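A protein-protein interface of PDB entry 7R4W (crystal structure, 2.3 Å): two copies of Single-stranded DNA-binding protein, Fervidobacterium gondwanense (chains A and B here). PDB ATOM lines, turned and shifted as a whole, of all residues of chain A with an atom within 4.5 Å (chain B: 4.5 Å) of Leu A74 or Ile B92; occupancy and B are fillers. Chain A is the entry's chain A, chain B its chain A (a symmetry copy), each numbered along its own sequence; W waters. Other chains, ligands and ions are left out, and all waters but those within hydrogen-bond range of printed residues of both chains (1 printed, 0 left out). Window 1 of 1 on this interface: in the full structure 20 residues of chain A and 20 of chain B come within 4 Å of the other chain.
The side-chain carboxylate of Asp B44 lies within hydrogen-bond range of the backbone NH of Ile A76.
The guanidinium group of Arg A75 is in salt-bridge range of the side-chain carboxylate of Asp B44.
O of Glu A91 sits at hydrogen-bond distance from N of Arg A75 (2.9 Å).
N of Val B49 sits at hydrogen-bond distance from O of Ile B92 (2.9 Å).
ND2 of Asn A4 sits at hydrogen-bond distance from O of Leu A74 (2.8 Å).
The backbone NH (N) of Leu B8 lies within hydrogen-bond range of the backbone carbonyl oxygen (O) of Val B70 (2.7 Å).
ND2 of Asn A4 sits close to NH1 of Arg A75, 3.3 Å away.
The backbone NH (N) of Ile B92 sits at hydrogen-bond distance from the backbone carbonyl oxygen (O) of Arg B47 (3.1 Å).
CD2 of Leu B8 touches CA of Asn A4 (3.7 Å).
Asp B44 touches Leu A74.
Ile B46 touches Leu A74 (CG2 to CD2, 3.9 Å).
Leu A74 touches Ile B92 (CD2 to CD1, 3.96 Å).
Ile A92 touches Leu B74 (CD1 to CD2, 3.96 Å).
Leu A74 touches just these residues of chain B: Asp B44, Ile B46 and Ile B92.
Printed residues of chain B within 4 Å of Arg A75: Asp B44 (3.2 Å).
Of the printed residues of chain B, Ile A92 touches Leu B74.
Printed residues of chain A within 4 Å of Asp B44: Leu A74, Arg A75 and Ile A76.
Arg B47 touches none of the printed residues of chain A.
Of chain A, only Leu A74 (3.96 Å) comes within 4 Å of Ile B92.
The nearest printed residue of chain A that does not touch Ile B92 is Val A6 (6.9 Å).
The nearest printed residue of chain A that does not touch Leu B8 is Leu A74 (5.1 Å).
Of the 10 printed residues of chain A, 5 touch a printed residue of chain B.
Printed residues of chain A that touch a printed residue of chain B: Asn A4, Leu A74, Arg A75, Ile A76 and Ile A92.
Hydrophobic or aromatic side chains of chain A that line the printed part of chain B: Leu A74 and Ile A92.
Of the 15 printed residues of chain B, 5 touch a printed residue of chain A.
Printed residues of chain B that touch a printed residue of chain A: Leu B8, Asp B44, Ile B46, Leu B74 and Ile B92.
Leu A74 touches Ile B92, and with the chains exchanged Ile A92 touches Leu B74.
Positions printed for both chains: 6, 72, 73, 74, 91 and 92.
Water W1 lies within hydrogen-bond range of the side-chain carboxylate (OD2) of Asp B44, the side-chain amide nitrogen (ND2) of Asn A4 and the guanidinium group (NH1) of Arg A75.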
ATOM      1  N   ASN A   4     -20.387   0.728 -31.282  1.00  0.00           N
ATOM      2  CA  ASN A   4     -20.304   1.599 -30.110  1.00  0.00           C
ATOM      3  C   ASN A   4     -21.734   1.940 -29.714  1.00  0.00           C
ATOM      4  O   ASN A   4     -22.361   2.758 -30.451  1.00  0.00           O
ATOM      5  CB  ASN A   4     -19.456   2.824 -30.476  1.00  0.00           C
ATOM      6  CG  ASN A   4     -19.152   3.771 -29.327  1.00  0.00           C
ATOM      7  OD1 ASN A   4     -19.924   3.853 -28.369  1.00  0.00           O
ATOM      8  ND2 ASN A   4     -18.031   4.487 -29.442  1.00  0.00           N
ATOM      9  N   VAL A   6     -24.134   2.841 -26.101  1.00  0.00           N
ATOM     10  CA  VAL A   6     -24.256   3.102 -24.635  1.00  0.00           C
ATOM     11  C   VAL A   6     -25.733   3.340 -24.308  1.00  0.00           C
ATOM     12  O   VAL A   6     -26.466   4.119 -25.044  1.00  0.00           O
ATOM     13  CB  VAL A   6     -23.459   4.362 -24.282  1.00  0.00           C
ATOM     14  CG1 VAL A   6     -23.367   4.581 -22.787  1.00  0.00           C
ATOM     15  CG2 VAL A   6     -22.062   4.356 -24.923  1.00  0.00           C
ATOM     16  N   GLY A  72     -26.636   6.462 -26.942  1.00  0.00           N
ATOM     17  CA  GLY A  72     -25.774   7.058 -27.971  1.00  0.00           C
ATOM     18  C   GLY A  72     -24.461   6.322 -28.008  1.00  0.00           C
ATOM     19  O   GLY A  72     -24.464   5.118 -27.691  1.00  0.00           O
ATOM     20  N   LYS A  73     -23.382   7.047 -28.288  1.00  0.00           N
ATOM     21  CA  LYS A  73     -22.044   6.475 -28.484  1.00  0.00           C
ATOM     22  C   LYS A  73     -21.073   7.140 -27.544  1.00  0.00           C
ATOM     23  O   LYS A  73     -21.149   8.367 -27.410  1.00  0.00           O
ATOM     24  CB  LYS A  73     -21.729   6.668 -29.955  1.00  0.00           C
ATOM     25  CG  LYS A  73     -22.814   6.083 -30.841  1.00  0.00           C
ATOM     26  CD  LYS A  73     -22.459   6.047 -32.294  1.00  0.00           C
ATOM     27  CE  LYS A  73     -23.527   5.348 -33.101  1.00  0.00           C
ATOM     28  NZ  LYS A  73     -24.654   6.278 -33.388  1.00  0.00           N
ATOM     29  N   LEU A  74     -20.172   6.348 -26.974  1.00  0.00           N
ATOM     30  CA  LEU A  74     -19.001   6.840 -26.200  1.00  0.00           C
ATOM     31  C   LEU A  74     -17.990   7.536 -27.148  1.00  0.00           C
ATOM     32  O   LEU A  74     -17.605   6.899 -28.156  1.00  0.00           O
ATOM     33  CB  LEU A  74     -18.405   5.629 -25.478  1.00  0.00           C
ATOM     34  CG  LEU A  74     -17.202   5.941 -24.601  1.00  0.00           C
ATOM     35  CD1 LEU A  74     -17.547   7.089 -23.665  1.00  0.00           C
ATOM     36  CD2 LEU A  74     -16.804   4.728 -23.782  1.00  0.00           C
ATOM     37  N   ARG A  75     -17.637   8.805 -26.869  1.00  0.00           N
ATOM     38  CA  ARG A  75     -16.661   9.677 -27.602  1.00  0.00           C
ATOM     39  C   ARG A  75     -15.596  10.131 -26.602  1.00  0.00           C
ATOM     40  O   ARG A  75     -15.923  10.478 -25.470  1.00  0.00           O
ATOM     41  CB  ARG A  75     -17.394  10.844 -28.269  1.00  0.00           C
ATOM     42  CG  ARG A  75     -18.698  10.372 -28.918  1.00  0.00           C
ATOM     43  CD  ARG A  75     -18.265  10.096 -30.300  1.00  0.00           C
ATOM     44  NE  ARG A  75     -19.092   9.497 -31.314  1.00  0.00           N
ATOM     45  CZ  ARG A  75     -18.963   8.241 -31.696  1.00  0.00           C
ATOM     46  NH1 ARG A  75     -18.295   7.342 -30.980  1.00  0.00           N
ATOM     47  NH2 ARG A  75     -19.562   7.880 -32.799  1.00  0.00           N
ATOM     48  N   ILE A  76     -14.334   9.954 -26.936  1.00  0.00           N
ATOM     49  CA  ILE A  76     -13.244  10.373 -26.032  1.00  0.00           C
ATOM     50  C   ILE A  76     -12.635  11.616 -26.665  1.00  0.00           C
ATOM     51  O   ILE A  76     -12.051  11.489 -27.706  1.00  0.00           O
ATOM     52  CB  ILE A  76     -12.223   9.262 -25.826  1.00  0.00           C
ATOM     53  CG1 ILE A  76     -12.819   8.026 -25.174  1.00  0.00           C
ATOM     54  CG2 ILE A  76     -11.066   9.787 -25.002  1.00  0.00           C
ATOM     55  CD1 ILE A  76     -13.382   8.295 -23.831  1.00  0.00           C
ATOM     56  N   VAL A  90     -14.728  12.633 -21.596  1.00  0.00           N
ATOM     57  CA  VAL A  90     -15.703  11.609 -21.974  1.00  0.00           C
ATOM     58  C   VAL A  90     -17.081  12.189 -22.107  1.00  0.00           C
ATOM     59  O   VAL A  90     -17.571  12.822 -21.179  1.00  0.00           O
ATOM     60  CB  VAL A  90     -15.694  10.554 -20.899  1.00  0.00           C
ATOM     61  CG1 VAL A  90     -16.397   9.318 -21.388  1.00  0.00           C
ATOM     62  CG2 VAL A  90     -14.242  10.342 -20.595  1.00  0.00           C
ATOM     63  N   GLU A  91     -17.734  11.745 -23.151  1.00  0.00           N
ATOM     64  CA  GLU A  91     -19.039  12.275 -23.549  1.00  0.00           C
ATOM     65  C   GLU A  91     -19.826  11.147 -24.216  1.00  0.00           C
ATOM     66  O   GLU A  91     -19.226  10.400 -24.996  1.00  0.00           O
ATOM     67  CB  GLU A  91     -18.843  13.340 -24.620  1.00  0.00           C
ATOM     68  CG  GLU A  91     -18.054  14.526 -24.190  1.00  0.00           C
ATOM     69  CD  GLU A  91     -17.958  15.557 -25.296  1.00  0.00           C
ATOM     70  OE1 GLU A  91     -18.066  15.178 -26.489  1.00  0.00           O
ATOM     71  OE2 GLU A  91     -17.775  16.729 -24.967  1.00  0.00           O
ATOM     72  N   ILE A  92     -21.128  11.112 -23.996  1.00  0.00           N
ATOM     73  CA  ILE A  92     -22.058  10.332 -24.819  1.00  0.00           C
ATOM     74  C   ILE A  92     -22.676  11.287 -25.819  1.00  0.00           C
ATOM     75  O   ILE A  92     -23.268  12.263 -25.403  1.00  0.00           O
ATOM     76  CB  ILE A  92     -23.106   9.629 -23.953  1.00  0.00           C
ATOM     77  CG1 ILE A  92     -22.495   8.834 -22.800  1.00  0.00           C
ATOM     78  CG2 ILE A  92     -23.928   8.739 -24.853  1.00  0.00           C
ATOM     79  CD1 ILE A  92     -21.301   8.011 -23.189  1.00  0.00           C
ATOM     80  N   VAL B   6     -22.923  -0.621 -21.820  1.00  0.00           N
ATOM     81  CA  VAL B   6     -22.064  -0.252 -22.985  1.00  0.00           C
ATOM     82  C   VAL B   6     -21.790  -1.519 -23.803  1.00  0.00           C
ATOM     83  O   VAL B   6     -21.446  -2.629 -23.225  1.00  0.00           O
ATOM     84  CB  VAL B   6     -20.733   0.305 -22.470  1.00  0.00           C
ATOM     85  CG1 VAL B   6     -19.888   0.886 -23.583  1.00  0.00           C
ATOM     86  CG2 VAL B   6     -20.937   1.329 -21.343  1.00  0.00           C
ATOM     87  N   LEU B   8     -19.422  -2.616 -27.103  1.00  0.00           N
ATOM     88  CA  LEU B   8     -18.380  -2.179 -28.069  1.00  0.00           C
ATOM     89  C   LEU B   8     -17.857  -3.349 -28.871  1.00  0.00           C
ATOM     90  O   LEU B   8     -17.607  -4.450 -28.318  1.00  0.00           O
ATOM     91  CB  LEU B   8     -17.213  -1.575 -27.290  1.00  0.00           C
ATOM     92  CG  LEU B   8     -17.520  -0.317 -26.481  1.00  0.00           C
ATOM     93  CD1 LEU B   8     -16.324   0.035 -25.623  1.00  0.00           C
ATOM     94  CD2 LEU B   8     -17.891   0.862 -27.385  1.00  0.00           C
ATOM     95  N   ASP B  44     -12.041   6.161 -31.298  1.00  0.00           N
ATOM     96  CA  ASP B  44     -11.954   6.314 -29.832  1.00  0.00           C
ATOM     97  C   ASP B  44     -11.185   5.102 -29.343  1.00  0.00           C
ATOM     98  O   ASP B  44     -11.472   4.003 -29.777  1.00  0.00           O
ATOM     99  CB  ASP B  44     -13.334   6.435 -29.177  1.00  0.00           C
ATOM    100  CG  ASP B  44     -14.151   7.564 -29.790  1.00  0.00           C
ATOM    101  OD1 ASP B  44     -13.811   8.718 -29.519  1.00  0.00           O
ATOM    102  OD2 ASP B  44     -15.092   7.286 -30.580  1.00  0.00           O
ATOM    103  N   ILE B  46     -10.596   3.029 -26.063  1.00  0.00           N
ATOM    104  CA  ILE B  46     -11.340   2.984 -24.785  1.00  0.00           C
ATOM    105  C   ILE B  46     -10.698   1.921 -23.892  1.00  0.00           C
ATOM    106  O   ILE B  46     -10.555   0.785 -24.342  1.00  0.00           O
ATOM    107  CB  ILE B  46     -12.811   2.702 -25.130  1.00  0.00           C
ATOM    108  CG1 ILE B  46     -13.403   3.814 -26.007  1.00  0.00           C
ATOM    109  CG2 ILE B  46     -13.620   2.473 -23.878  1.00  0.00           C
ATOM    110  CD1 ILE B  46     -14.628   3.412 -26.831  1.00  0.00           C
ATOM    111  N   ARG B  47     -10.364   2.264 -22.654  1.00  0.00           N
ATOM    112  CA  ARG B  47      -9.717   1.300 -21.749  1.00  0.00           C
ATOM    113  C   ARG B  47     -10.817   0.350 -21.348  1.00  0.00           C
ATOM    114  O   ARG B  47     -11.881   0.858 -20.948  1.00  0.00           O
ATOM    115  CB  ARG B  47      -9.136   1.957 -20.490  1.00  0.00           C
ATOM    116  CG  ARG B  47      -8.371   0.959 -19.615  1.00  0.00           C
ATOM    117  CD  ARG B  47      -7.916   1.473 -18.238  1.00  0.00           C
ATOM    118  NE  ARG B  47      -7.034   2.644 -18.264  1.00  0.00           N
ATOM    119  CZ  ARG B  47      -7.255   3.833 -17.671  1.00  0.00           C
ATOM    120  NH1 ARG B  47      -8.344   4.073 -16.956  1.00  0.00           N
ATOM    121  NH2 ARG B  47      -6.351   4.794 -17.782  1.00  0.00           N
ATOM    122  N   ILE B  48     -10.540  -0.945 -21.403  1.00  0.00           N
ATOM    123  CA  ILE B  48     -11.408  -1.999 -20.829  1.00  0.00           C
ATOM    124  C   ILE B  48     -10.700  -2.575 -19.606  1.00  0.00           C
ATOM    125  O   ILE B  48      -9.483  -2.763 -19.655  1.00  0.00           O
ATOM    126  CB  ILE B  48     -11.714  -3.078 -21.883  1.00  0.00           C
ATOM    127  CG1 ILE B  48     -12.117  -2.497 -23.247  1.00  0.00           C
ATOM    128  CG2 ILE B  48     -12.745  -4.040 -21.325  1.00  0.00           C
ATOM    129  CD1 ILE B  48     -13.327  -1.617 -23.179  1.00  0.00           C
ATOM    130  N   VAL B  49     -11.471  -2.915 -18.587  1.00  0.00           N
ATOM    131  CA  VAL B  49     -11.005  -3.526 -17.318  1.00  0.00           C
ATOM    132  C   VAL B  49     -11.827  -4.772 -17.097  1.00  0.00           C
ATOM    133  O   VAL B  49     -13.057  -4.639 -17.064  1.00  0.00           O
ATOM    134  CB  VAL B  49     -11.221  -2.579 -16.129  1.00  0.00           C
ATOM    135  CG1 VAL B  49     -10.641  -3.161 -14.852  1.00  0.00           C
ATOM    136  CG2 VAL B  49     -10.681  -1.180 -16.425  1.00  0.00           C
ATOM    137  N   VAL B  70     -17.126  -6.431 -26.335  1.00  0.00           N
ATOM    138  CA  VAL B  70     -17.173  -6.241 -24.872  1.00  0.00           C
ATOM    139  C   VAL B  70     -18.495  -5.565 -24.552  1.00  0.00           C
ATOM    140  O   VAL B  70     -18.872  -4.556 -25.281  1.00  0.00           O
ATOM    141  CB  VAL B  70     -16.006  -5.328 -24.459  1.00  0.00           C
ATOM    142  CG1 VAL B  70     -16.101  -4.915 -23.006  1.00  0.00           C
ATOM    143  CG2 VAL B  70     -14.677  -5.997 -24.724  1.00  0.00           C
ATOM    144  N   GLY B  72     -20.160  -4.019 -20.872  1.00  0.00           N
ATOM    145  CA  GLY B  72     -20.018  -3.758 -19.434  1.00  0.00           C
ATOM    146  C   GLY B  72     -20.626  -2.419 -19.109  1.00  0.00           C
ATOM    147  O   GLY B  72     -21.574  -2.028 -19.814  1.00  0.00           O
ATOM    148  N   LYS B  73     -20.033  -1.717 -18.148  1.00  0.00           N
ATOM    149  CA  LYS B  73     -20.559  -0.452 -17.621  1.00  0.00           C
ATOM    150  C   LYS B  73     -19.502   0.616 -17.733  1.00  0.00           C
ATOM    151  O   LYS B  73     -18.343   0.313 -17.426  1.00  0.00           O
ATOM    152  CB  LYS B  73     -21.001  -0.753 -16.202  1.00  0.00           C
ATOM    153  CG  LYS B  73     -21.969  -1.921 -16.152  1.00  0.00           C
ATOM    154  CD  LYS B  73     -22.607  -2.126 -14.815  1.00  0.00           C
ATOM    155  CE  LYS B  73     -23.642  -3.224 -14.866  1.00  0.00           C
ATOM    156  NZ  LYS B  73     -22.991  -4.559 -14.772  1.00  0.00           N
ATOM    157  N   LEU B  74     -19.920   1.820 -18.107  1.00  0.00           N
ATOM    158  CA  LEU B  74     -19.079   3.046 -18.060  1.00  0.00           C
ATOM    159  C   LEU B  74     -18.805   3.448 -16.588  1.00  0.00           C
ATOM    160  O   LEU B  74     -19.791   3.571 -15.825  1.00  0.00           O
ATOM    161  CB  LEU B  74     -19.827   4.127 -18.845  1.00  0.00           C
ATOM    162  CG  LEU B  74     -19.103   5.461 -18.935  1.00  0.00           C
ATOM    163  CD1 LEU B  74     -17.684   5.229 -19.434  1.00  0.00           C
ATOM    164  CD2 LEU B  74     -19.821   6.400 -19.885  1.00  0.00           C
ATOM    165  N   GLU B  91     -13.279   4.176 -18.228  1.00  0.00           N
ATOM    166  CA  GLU B  91     -13.044   2.732 -18.265  1.00  0.00           C
ATOM    167  C   GLU B  91     -14.390   2.038 -18.469  1.00  0.00           C
ATOM    168  O   GLU B  91     -15.366   2.464 -17.842  1.00  0.00           O
ATOM    169  CB  GLU B  91     -12.534   2.269 -16.907  1.00  0.00           C
ATOM    170  CG  GLU B  91     -11.238   2.865 -16.486  1.00  0.00           C
ATOM    171  CD  GLU B  91     -10.779   2.308 -15.154  1.00  0.00           C
ATOM    172  OE1 GLU B  91     -11.640   1.859 -14.356  1.00  0.00           O
ATOM    173  OE2 GLU B  91      -9.572   2.323 -14.916  1.00  0.00           O
ATOM    174  N   ILE B  92     -14.400   0.954 -19.224  1.00  0.00           N
ATOM    175  CA  ILE B  92     -15.508  -0.007 -19.231  1.00  0.00           C
ATOM    176  C   ILE B  92     -15.112  -1.151 -18.322  1.00  0.00           C
ATOM    177  O   ILE B  92     -14.086  -1.756 -18.561  1.00  0.00           O
ATOM    178  CB  ILE B  92     -15.826  -0.471 -20.655  1.00  0.00           C
ATOM    179  CG1 ILE B  92     -16.013   0.686 -21.635  1.00  0.00           C
ATOM    180  CG2 ILE B  92     -17.061  -1.337 -20.593  1.00  0.00           C
ATOM    181  CD1 ILE B  92     -16.856   1.809 -21.102  1.00  0.00           C
ATOM    182  N   TRP B  93     -15.909  -1.408 -17.303  1.00  0.00           N
ATOM    183  CA  TRP B  93     -15.800  -2.648 -16.516  1.00  0.00           C
ATOM    184  C   TRP B  93     -16.613  -3.700 -17.245  1.00  0.00           C
ATOM    185  O   TRP B  93     -17.856  -3.607 -17.258  1.00  0.00           O
ATOM    186  CB  TRP B  93     -16.278  -2.445 -15.072  1.00  0.00           C
ATOM    187  CG  TRP B  93     -15.416  -1.470 -14.326  1.00  0.00           C
ATOM    188  CD1 TRP B  93     -14.411  -0.688 -14.819  1.00  0.00           C
ATOM    189  CD2 TRP B  93     -15.517  -1.153 -12.949  1.00  0.00           C
ATOM    190  NE1 TRP B  93     -13.870   0.074 -13.835  1.00  0.00           N
ATOM    191  CE2 TRP B  93     -14.510  -0.216 -12.669  1.00  0.00           C
ATOM    192  CE3 TRP B  93     -16.339  -1.601 -11.920  1.00  0.00           C
ATOM    193  CZ2 TRP B  93     -14.328   0.301 -11.392  1.00  0.00           C
ATOM    194  CZ3 TRP B  93     -16.151  -1.101 -10.657  1.00  0.00           C
ATOM    195  CH2 TRP B  93     -15.145  -0.175 -10.399  1.00  0.00           C
ATOM    196  N   ALA B  94     -15.903  -4.623 -17.868  1.00  0.00           N
ATOM    197  CA  ALA B  94     -16.475  -5.641 -18.754  1.00  0.00           C
ATOM    198  C   ALA B  94     -17.378  -6.555 -17.927  1.00  0.00           C
ATOM    199  O   ALA B  94     -16.952  -6.963 -16.868  1.00  0.00           O
ATOM    200  CB  ALA B  94     -15.352  -6.380 -19.411  1.00  0.00           C
HETATM  201  O   HOH W   1     -16.121   5.125 -31.438  1.00  0.00           O
